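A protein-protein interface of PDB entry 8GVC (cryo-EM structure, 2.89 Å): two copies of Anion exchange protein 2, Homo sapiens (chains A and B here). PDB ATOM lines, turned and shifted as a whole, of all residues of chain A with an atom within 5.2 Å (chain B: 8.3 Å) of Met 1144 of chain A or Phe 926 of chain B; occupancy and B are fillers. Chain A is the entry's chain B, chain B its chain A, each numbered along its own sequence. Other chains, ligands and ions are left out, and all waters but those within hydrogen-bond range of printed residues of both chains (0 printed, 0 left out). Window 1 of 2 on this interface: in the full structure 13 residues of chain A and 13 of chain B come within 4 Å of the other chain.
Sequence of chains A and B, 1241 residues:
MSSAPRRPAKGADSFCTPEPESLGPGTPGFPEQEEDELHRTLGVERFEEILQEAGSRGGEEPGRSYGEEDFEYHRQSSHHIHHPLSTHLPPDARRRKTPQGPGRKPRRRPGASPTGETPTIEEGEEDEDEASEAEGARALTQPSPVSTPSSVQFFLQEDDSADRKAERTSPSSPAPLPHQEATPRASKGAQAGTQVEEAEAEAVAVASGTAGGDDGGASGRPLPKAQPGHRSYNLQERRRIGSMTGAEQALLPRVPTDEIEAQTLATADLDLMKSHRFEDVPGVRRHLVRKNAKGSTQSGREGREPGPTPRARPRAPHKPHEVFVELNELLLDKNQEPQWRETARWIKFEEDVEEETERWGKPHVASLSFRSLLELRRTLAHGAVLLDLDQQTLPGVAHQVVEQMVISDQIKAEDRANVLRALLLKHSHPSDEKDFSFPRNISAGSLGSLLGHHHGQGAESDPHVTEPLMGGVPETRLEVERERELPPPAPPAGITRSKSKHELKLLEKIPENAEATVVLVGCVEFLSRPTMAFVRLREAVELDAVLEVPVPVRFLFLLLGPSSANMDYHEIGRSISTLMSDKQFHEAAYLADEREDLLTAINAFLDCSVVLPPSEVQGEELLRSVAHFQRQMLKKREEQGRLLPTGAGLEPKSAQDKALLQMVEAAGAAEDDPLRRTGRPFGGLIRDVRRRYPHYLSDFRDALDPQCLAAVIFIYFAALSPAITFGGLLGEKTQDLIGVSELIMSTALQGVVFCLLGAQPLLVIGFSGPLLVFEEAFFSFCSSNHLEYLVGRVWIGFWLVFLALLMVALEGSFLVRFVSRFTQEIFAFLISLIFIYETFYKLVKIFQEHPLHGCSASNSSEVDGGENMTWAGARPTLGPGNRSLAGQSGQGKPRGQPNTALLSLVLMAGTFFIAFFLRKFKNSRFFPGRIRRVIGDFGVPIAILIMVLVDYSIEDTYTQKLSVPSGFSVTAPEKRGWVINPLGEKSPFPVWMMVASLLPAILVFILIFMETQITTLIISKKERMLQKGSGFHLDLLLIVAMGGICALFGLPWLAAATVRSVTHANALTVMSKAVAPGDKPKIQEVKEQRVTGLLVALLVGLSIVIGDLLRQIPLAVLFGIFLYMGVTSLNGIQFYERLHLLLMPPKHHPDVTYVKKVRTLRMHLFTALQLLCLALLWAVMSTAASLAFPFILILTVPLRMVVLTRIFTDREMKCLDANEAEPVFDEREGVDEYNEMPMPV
N of Phe 927 of chain B sits at hydrogen-bond distance from O of Leu 1143 of chain A.
OG of Ser 924 of chain B sits at hydrogen-bond distance from N of Phe 926 of chain B (3.5 Å). The backbone carbonyl oxygen of Phe 926 of chain B is in hydrogen-bond range of the guanidinium group of Arg 932 of chain B (2.9 Å). The backbone carbonyl oxygen (O) of Phe 927 of chain B is in hydrogen-bond range of the guanidinium group (NH1) of Arg 932 of chain B, at 2.7 Å.
Among the printed residues, merely in contact across the chains: Leu 1143 of chain A with Phe 926 of chain B, Met 1144 of chain A with Arg 925 of chain B, Met 1144 of chain A with Phe 926 of chain B, Pro 1145 of chain A with Arg 925 of chain B, Pro 1145 of chain A with Phe 927 of chain B and His 1148 of chain A with Arg 925 of chain B.
Met 1144 of chain A touches two residues of chain B. Of chain B, only Arg 925 (3.0 Å) and Phe 927 (3.95 Å) come within 4 Å of Pro 1145 of chain A. Of the printed residues of chain B, His 1148 of chain A touches Arg 925. Printed residues of chain A within 4 Å of Arg 925 of chain B: Met 1144, Pro 1145 and His 1148. Of the printed residues of chain A, Phe 926 of chain B touches Leu 1143 and Met 1144. Of the printed residues of chain A, Phe 927 of chain B touches Leu 1143 (3.2 Å) and Pro 1145 (3.95 Å).
Of the 15 printed residues of chain B, 3 touch a printed residue of chain A. Printed residues of chain B that touch a printed residue of chain A: Arg 925, Phe 926 and Phe 927. Hydrophobic or aromatic side chains of chain B that line the printed part of chain A: Phe 926. Of the 9 printed residues of chain A, 4 touch a printed residue of chain B.
No position is printed for both chains.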
ATOM      1  N   HIS A1140     -16.563  28.862  29.857  1.00  0.00           N
ATOM      2  CA  HIS A1140     -16.511  27.422  29.622  1.00  0.00           C
ATOM      3  C   HIS A1140     -17.909  26.822  29.583  1.00  0.00           C
ATOM      4  O   HIS A1140     -18.198  25.952  28.754  1.00  0.00           O
ATOM      5  CB  HIS A1140     -15.675  26.738  30.702  1.00  0.00           C
ATOM      6  CG  HIS A1140     -14.244  27.170  30.726  1.00  0.00           C
ATOM      7  ND1 HIS A1140     -13.357  26.748  31.692  1.00  0.00           N
ATOM      8  CD2 HIS A1140     -13.544  27.985  29.903  1.00  0.00           C
ATOM      9  CE1 HIS A1140     -12.173  27.285  31.464  1.00  0.00           C
ATOM     10  NE2 HIS A1140     -12.259  28.040  30.385  1.00  0.00           N
ATOM     11  N   LEU A1141     -18.793  27.281  30.469  1.00  0.00           N
ATOM     12  CA  LEU A1141     -20.129  26.706  30.572  1.00  0.00           C
ATOM     13  C   LEU A1141     -20.924  26.849  29.282  1.00  0.00           C
ATOM     14  O   LEU A1141     -21.911  26.131  29.095  1.00  0.00           O
ATOM     15  CB  LEU A1141     -20.881  27.357  31.732  1.00  0.00           C
ATOM     16  CG  LEU A1141     -20.687  26.717  33.108  1.00  0.00           C
ATOM     17  CD1 LEU A1141     -19.220  26.450  33.376  1.00  0.00           C
ATOM     18  CD2 LEU A1141     -21.263  27.607  34.191  1.00  0.00           C
ATOM     19  N   LEU A1142     -20.528  27.760  28.392  1.00  0.00           N
ATOM     20  CA  LEU A1142     -21.210  27.889  27.110  1.00  0.00           C
ATOM     21  C   LEU A1142     -21.018  26.664  26.226  1.00  0.00           C
ATOM     22  O   LEU A1142     -21.796  26.467  25.287  1.00  0.00           O
ATOM     23  CB  LEU A1142     -20.722  29.136  26.373  1.00  0.00           C
ATOM     24  CG  LEU A1142     -21.361  30.473  26.745  1.00  0.00           C
ATOM     25  CD1 LEU A1142     -20.580  31.617  26.131  1.00  0.00           C
ATOM     26  CD2 LEU A1142     -22.805  30.514  26.287  1.00  0.00           C
ATOM     27  N   LEU A1143     -20.003  25.844  26.498  1.00  0.00           N
ATOM     28  CA  LEU A1143     -19.718  24.661  25.699  1.00  0.00           C
ATOM     29  C   LEU A1143     -20.079  23.356  26.388  1.00  0.00           C
ATOM     30  O   LEU A1143     -20.444  22.396  25.707  1.00  0.00           O
ATOM     31  CB  LEU A1143     -18.233  24.622  25.317  1.00  0.00           C
ATOM     32  CG  LEU A1143     -17.618  25.948  24.864  1.00  0.00           C
ATOM     33  CD1 LEU A1143     -16.107  25.831  24.762  1.00  0.00           C
ATOM     34  CD2 LEU A1143     -18.215  26.395  23.539  1.00  0.00           C
ATOM     35  N   MET A1144     -19.987  23.295  27.713  1.00  0.00           N
ATOM     36  CA  MET A1144     -20.341  22.083  28.429  1.00  0.00           C
ATOM     37  C   MET A1144     -21.848  21.841  28.358  1.00  0.00           C
ATOM     38  O   MET A1144     -22.636  22.789  28.302  1.00  0.00           O
ATOM     39  CB  MET A1144     -19.905  22.178  29.887  1.00  0.00           C
ATOM     40  CG  MET A1144     -18.428  21.950  30.112  1.00  0.00           C
ATOM     41  SD  MET A1144     -17.963  22.181  31.835  1.00  0.00           S
ATOM     42  CE  MET A1144     -16.183  22.289  31.689  1.00  0.00           C
ATOM     43  N   PRO A1145     -22.274  20.577  28.353  1.00  0.00           N
ATOM     44  CA  PRO A1145     -23.705  20.294  28.424  1.00  0.00           C
ATOM     45  C   PRO A1145     -24.256  20.674  29.786  1.00  0.00           C
ATOM     46  O   PRO A1145     -23.525  20.670  30.790  1.00  0.00           O
ATOM     47  CB  PRO A1145     -23.779  18.775  28.188  1.00  0.00           C
ATOM     48  CG  PRO A1145     -22.446  18.269  28.588  1.00  0.00           C
ATOM     49  CD  PRO A1145     -21.468  19.350  28.249  1.00  0.00           C
ATOM     50  N   PRO A1146     -25.545  21.007  29.871  1.00  0.00           N
ATOM     51  CA  PRO A1146     -26.087  21.517  31.141  1.00  0.00           C
ATOM     52  C   PRO A1146     -25.965  20.551  32.305  1.00  0.00           C
ATOM     53  O   PRO A1146     -25.968  21.000  33.458  1.00  0.00           O
ATOM     54  CB  PRO A1146     -27.557  21.798  30.801  1.00  0.00           C
ATOM     55  CG  PRO A1146     -27.553  22.049  29.334  1.00  0.00           C
ATOM     56  CD  PRO A1146     -26.522  21.113  28.775  1.00  0.00           C
ATOM     57  N   HIS A1148     -23.365  18.792  33.147  1.00  0.00           N
ATOM     58  CA  HIS A1148     -22.009  18.770  33.676  1.00  0.00           C
ATOM     59  C   HIS A1148     -21.619  20.063  34.379  1.00  0.00           C
ATOM     60  O   HIS A1148     -20.474  20.187  34.823  1.00  0.00           O
ATOM     61  CB  HIS A1148     -21.010  18.477  32.554  1.00  0.00           C
ATOM     62  CG  HIS A1148     -20.991  17.045  32.119  1.00  0.00           C
ATOM     63  ND1 HIS A1148     -21.369  16.647  30.856  1.00  0.00           N
ATOM     64  CD2 HIS A1148     -20.638  15.917  32.778  1.00  0.00           C
ATOM     65  CE1 HIS A1148     -21.252  15.335  30.756  1.00  0.00           C
ATOM     66  NE2 HIS A1148     -20.810  14.868  31.909  1.00  0.00           N
ATOM     67  N   HIS A1149     -22.532  21.022  34.492  1.00  0.00           N
ATOM     68  CA  HIS A1149     -22.197  22.284  35.131  1.00  0.00           C
ATOM     69  C   HIS A1149     -21.841  22.046  36.597  1.00  0.00           C
ATOM     70  O   HIS A1149     -22.448  21.193  37.254  1.00  0.00           O
ATOM     71  CB  HIS A1149     -23.363  23.268  35.023  1.00  0.00           C
ATOM     72  CG  HIS A1149     -23.601  23.773  33.635  1.00  0.00           C
ATOM     73  ND1 HIS A1149     -22.682  23.624  32.620  1.00  0.00           N
ATOM     74  CD2 HIS A1149     -24.655  24.428  33.093  1.00  0.00           C
ATOM     75  CE1 HIS A1149     -23.159  24.164  31.513  1.00  0.00           C
ATOM     76  NE2 HIS A1149     -24.356  24.658  31.773  1.00  0.00           N
ATOM     77  N   PHE B 917      -3.666  16.157  22.109  1.00  0.00           N
ATOM     78  CA  PHE B 917      -4.751  17.032  22.540  1.00  0.00           C
ATOM     79  C   PHE B 917      -6.106  16.476  22.127  1.00  0.00           C
ATOM     80  O   PHE B 917      -7.063  16.514  22.908  1.00  0.00           O
ATOM     81  CB  PHE B 917      -4.557  18.437  21.973  1.00  0.00           C
ATOM     82  CG  PHE B 917      -5.810  19.268  21.978  1.00  0.00           C
ATOM     83  CD1 PHE B 917      -6.470  19.544  23.164  1.00  0.00           C
ATOM     84  CD2 PHE B 917      -6.332  19.765  20.797  1.00  0.00           C
ATOM     85  CE1 PHE B 917      -7.625  20.302  23.172  1.00  0.00           C
ATOM     86  CE2 PHE B 917      -7.488  20.524  20.799  1.00  0.00           C
ATOM     87  CZ  PHE B 917      -8.133  20.793  21.988  1.00  0.00           C
ATOM     88  N   LYS B 920      -7.023  13.695  24.460  1.00  0.00           N
ATOM     89  CA  LYS B 920      -7.492  14.175  25.759  1.00  0.00           C
ATOM     90  C   LYS B 920      -8.897  14.756  25.663  1.00  0.00           C
ATOM     91  O   LYS B 920      -9.709  14.585  26.579  1.00  0.00           O
ATOM     92  CB  LYS B 920      -6.525  15.214  26.323  1.00  0.00           C
ATOM     93  CG  LYS B 920      -5.272  14.622  26.938  1.00  0.00           C
ATOM     94  CD  LYS B 920      -4.468  15.682  27.664  1.00  0.00           C
ATOM     95  CE  LYS B 920      -3.223  15.086  28.297  1.00  0.00           C
ATOM     96  NZ  LYS B 920      -3.556  13.980  29.235  1.00  0.00           N
ATOM     97  N   PHE B 921      -9.201  15.454  24.569  1.00  0.00           N
ATOM     98  CA  PHE B 921     -10.520  16.051  24.398  1.00  0.00           C
ATOM     99  C   PHE B 921     -11.631  15.008  24.361  1.00  0.00           C
ATOM    100  O   PHE B 921     -12.794  15.349  24.599  1.00  0.00           O
ATOM    101  CB  PHE B 921     -10.538  16.893  23.121  1.00  0.00           C
ATOM    102  CG  PHE B 921     -11.913  17.255  22.644  1.00  0.00           C
ATOM    103  CD1 PHE B 921     -12.667  18.204  23.310  1.00  0.00           C
ATOM    104  CD2 PHE B 921     -12.450  16.652  21.521  1.00  0.00           C
ATOM    105  CE1 PHE B 921     -13.931  18.540  22.869  1.00  0.00           C
ATOM    106  CE2 PHE B 921     -13.713  16.985  21.076  1.00  0.00           C
ATOM    107  CZ  PHE B 921     -14.454  17.929  21.752  1.00  0.00           C
ATOM    108  N   LYS B 922     -11.301  13.747  24.078  1.00  0.00           N
ATOM    109  CA  LYS B 922     -12.329  12.716  23.963  1.00  0.00           C
ATOM    110  C   LYS B 922     -12.977  12.416  25.310  1.00  0.00           C
ATOM    111  O   LYS B 922     -14.185  12.160  25.378  1.00  0.00           O
ATOM    112  CB  LYS B 922     -11.726  11.447  23.362  1.00  0.00           C
ATOM    113  CG  LYS B 922     -12.711  10.309  23.185  1.00  0.00           C
ATOM    114  CD  LYS B 922     -12.049   9.126  22.506  1.00  0.00           C
ATOM    115  CE  LYS B 922     -10.949   8.543  23.376  1.00  0.00           C
ATOM    116  NZ  LYS B 922     -10.257   7.406  22.711  1.00  0.00           N
ATOM    117  N   ASN B 923     -12.197  12.434  26.387  1.00  0.00           N
ATOM    118  CA  ASN B 923     -12.697  12.124  27.720  1.00  0.00           C
ATOM    119  C   ASN B 923     -13.153  13.356  28.491  1.00  0.00           C
ATOM    120  O   ASN B 923     -13.512  13.233  29.666  1.00  0.00           O
ATOM    121  CB  ASN B 923     -11.623  11.389  28.527  1.00  0.00           C
ATOM    122  CG  ASN B 923     -10.801  10.443  27.677  1.00  0.00           C
ATOM    123  OD1 ASN B 923     -11.342   9.662  26.896  1.00  0.00           O
ATOM    124  ND2 ASN B 923      -9.483  10.506  27.829  1.00  0.00           N
ATOM    125  N   SER B 924     -13.153  14.529  27.867  1.00  0.00           N
ATOM    126  CA  SER B 924     -13.496  15.766  28.554  1.00  0.00           C
ATOM    127  C   SER B 924     -15.007  15.870  28.746  1.00  0.00           C
ATOM    128  O   SER B 924     -15.761  14.929  28.483  1.00  0.00           O
ATOM    129  CB  SER B 924     -12.947  16.963  27.784  1.00  0.00           C
ATOM    130  OG  SER B 924     -13.695  17.189  26.604  1.00  0.00           O
ATOM    131  N   ARG B 925     -15.466  17.031  29.217  1.00  0.00           N
ATOM    132  CA  ARG B 925     -16.881  17.289  29.457  1.00  0.00           C
ATOM    133  C   ARG B 925     -17.462  18.323  28.501  1.00  0.00           C
ATOM    134  O   ARG B 925     -18.524  18.887  28.774  1.00  0.00           O
ATOM    135  CB  ARG B 925     -17.091  17.720  30.907  1.00  0.00           C
ATOM    136  CG  ARG B 925     -16.854  16.618  31.925  1.00  0.00           C
ATOM    137  CD  ARG B 925     -17.380  17.012  33.294  1.00  0.00           C
ATOM    138  NE  ARG B 925     -16.687  18.173  33.836  1.00  0.00           N
ATOM    139  CZ  ARG B 925     -15.554  18.118  34.521  1.00  0.00           C
ATOM    140  NH1 ARG B 925     -14.952  16.965  34.766  1.00  0.00           N
ATOM    141  NH2 ARG B 925     -15.012  19.245  34.973  1.00  0.00           N
ATOM    142  N   PHE B 926     -16.786  18.587  27.387  1.00  0.00           N
ATOM    143  CA  PHE B 926     -17.216  19.589  26.425  1.00  0.00           C
ATOM    144  C   PHE B 926     -17.988  18.962  25.270  1.00  0.00           C
ATOM    145  O   PHE B 926     -17.710  17.836  24.852  1.00  0.00           O
ATOM    146  CB  PHE B 926     -16.009  20.355  25.880  1.00  0.00           C
ATOM    147  CG  PHE B 926     -15.266  21.136  26.923  1.00  0.00           C
ATOM    148  CD1 PHE B 926     -15.624  22.440  27.216  1.00  0.00           C
ATOM    149  CD2 PHE B 926     -14.208  20.569  27.609  1.00  0.00           C
ATOM    150  CE1 PHE B 926     -14.943  23.160  28.173  1.00  0.00           C
ATOM    151  CE2 PHE B 926     -13.523  21.286  28.567  1.00  0.00           C
ATOM    152  CZ  PHE B 926     -13.891  22.582  28.849  1.00  0.00           C
ATOM    153  N   PHE B 927     -18.966  19.707  24.761  1.00  0.00           N
ATOM    154  CA  PHE B 927     -19.737  19.297  23.593  1.00  0.00           C
ATOM    155  C   PHE B 927     -20.622  18.098  23.914  1.00  0.00           C
ATOM    156  O   PHE B 927     -20.436  17.443  24.947  1.00  0.00           O
ATOM    157  CB  PHE B 927     -18.804  18.961  22.428  1.00  0.00           C
ATOM    158  CG  PHE B 927     -18.139  20.160  21.815  1.00  0.00           C
ATOM    159  CD1 PHE B 927     -17.187  20.877  22.516  1.00  0.00           C
ATOM    160  CD2 PHE B 927     -18.461  20.563  20.531  1.00  0.00           C
ATOM    161  CE1 PHE B 927     -16.572  21.976  21.953  1.00  0.00           C
ATOM    162  CE2 PHE B 927     -17.849  21.663  19.963  1.00  0.00           C
ATOM    163  CZ  PHE B 927     -16.904  22.370  20.677  1.00  0.00           C
ATOM    164  N   PRO B 928     -21.592  17.782  23.058  1.00  0.00           N
ATOM    165  CA  PRO B 928     -22.409  16.584  23.281  1.00  0.00           C
ATOM    166  C   PRO B 928     -21.562  15.322  23.217  1.00  0.00           C
ATOM    167  O   PRO B 928     -20.521  15.278  22.559  1.00  0.00           O
ATOM    168  CB  PRO B 928     -23.432  16.633  22.141  1.00  0.00           C
ATOM    169  CG  PRO B 928     -23.444  18.058  21.693  1.00  0.00           C
ATOM    170  CD  PRO B 928     -22.050  18.558  21.895  1.00  0.00           C
ATOM    171  N   GLY B 929     -22.023  14.286  23.917  1.00  0.00           N
ATOM    172  CA  GLY B 929     -21.237  13.067  24.018  1.00  0.00           C
ATOM    173  C   GLY B 929     -20.962  12.418  22.675  1.00  0.00           C
ATOM    174  O   GLY B 929     -19.842  11.977  22.406  1.00  0.00           O
ATOM    175  N   ARG B 930     -21.978  12.348  21.812  1.00  0.00           N
ATOM    176  CA  ARG B 930     -21.807  11.683  20.525  1.00  0.00           C
ATOM    177  C   ARG B 930     -20.766  12.394  19.669  1.00  0.00           C
ATOM    178  O   ARG B 930     -19.832  11.767  19.154  1.00  0.00           O
ATOM    179  CB  ARG B 930     -23.148  11.611  19.794  1.00  0.00           C
ATOM    180  CG  ARG B 930     -24.191  10.760  20.498  1.00  0.00           C
ATOM    181  CD  ARG B 930     -23.893   9.278  20.334  1.00  0.00           C
ATOM    182  NE  ARG B 930     -24.071   8.836  18.956  1.00  0.00           N
ATOM    183  CZ  ARG B 930     -25.238   8.507  18.419  1.00  0.00           C
ATOM    184  NH1 ARG B 930     -26.359   8.553  19.121  1.00  0.00           N
ATOM    185  NH2 ARG B 930     -25.282   8.120  17.147  1.00  0.00           N
ATOM    186  N   ILE B 931     -20.915  13.710  19.502  1.00  0.00           N
ATOM    187  CA  ILE B 931     -19.967  14.474  18.698  1.00  0.00           C
ATOM    188  C   ILE B 931     -18.579  14.417  19.315  1.00  0.00           C
ATOM    189  O   ILE B 931     -17.571  14.276  18.610  1.00  0.00           O
ATOM    190  CB  ILE B 931     -20.454  15.925  18.535  1.00  0.00           C
ATOM    191  CG1 ILE B 931     -21.778  15.958  17.772  1.00  0.00           C
ATOM    192  CG2 ILE B 931     -19.400  16.762  17.833  1.00  0.00           C
ATOM    193  CD1 ILE B 931     -22.460  17.306  17.787  1.00  0.00           C
ATOM    194  N   ARG B 932     -18.502  14.542  20.640  1.00  0.00           N
ATOM    195  CA  ARG B 932     -17.209  14.497  21.310  1.00  0.00           C
ATOM    196  C   ARG B 932     -16.497  13.179  21.043  1.00  0.00           C
ATOM    197  O   ARG B 932     -15.309  13.166  20.709  1.00  0.00           O
ATOM    198  CB  ARG B 932     -17.394  14.718  22.809  1.00  0.00           C
ATOM    199  CG  ARG B 932     -16.151  14.475  23.636  1.00  0.00           C
ATOM    200  CD  ARG B 932     -16.306  15.057  25.029  1.00  0.00           C
ATOM    201  NE  ARG B 932     -17.035  14.159  25.917  1.00  0.00           N
ATOM    202  CZ  ARG B 932     -18.273  14.369  26.343  1.00  0.00           C
ATOM    203  NH1 ARG B 932     -18.960  15.435  25.972  1.00  0.00           N
ATOM    204  NH2 ARG B 932     -18.835  13.483  27.160  1.00  0.00           N
ATOM    205  N   ARG B 933     -17.210  12.057  21.170  1.00  0.00           N
ATOM    206  CA  ARG B 933     -16.589  10.757  20.930  1.00  0.00           C
ATOM    207  C   ARG B 933     -16.191  10.591  19.467  1.00  0.00           C
ATOM    208  O   ARG B 933     -15.103  10.081  19.165  1.00  0.00           O
ATOM    209  CB  ARG B 933     -17.535   9.638  21.360  1.00  0.00           C
ATOM    210  CG  ARG B 933     -17.400   9.249  22.822  1.00  0.00           C
ATOM    211  CD  ARG B 933     -18.339   8.109  23.183  1.00  0.00           C
ATOM    212  NE  ARG B 933     -19.570   8.581  23.809  1.00  0.00           N
ATOM    213  CZ  ARG B 933     -19.620   9.326  24.905  1.00  0.00           C
ATOM    214  NH1 ARG B 933     -18.520   9.703  25.537  1.00  0.00           N
ATOM    215  NH2 ARG B 933     -20.804   9.701  25.380  1.00  0.00           N
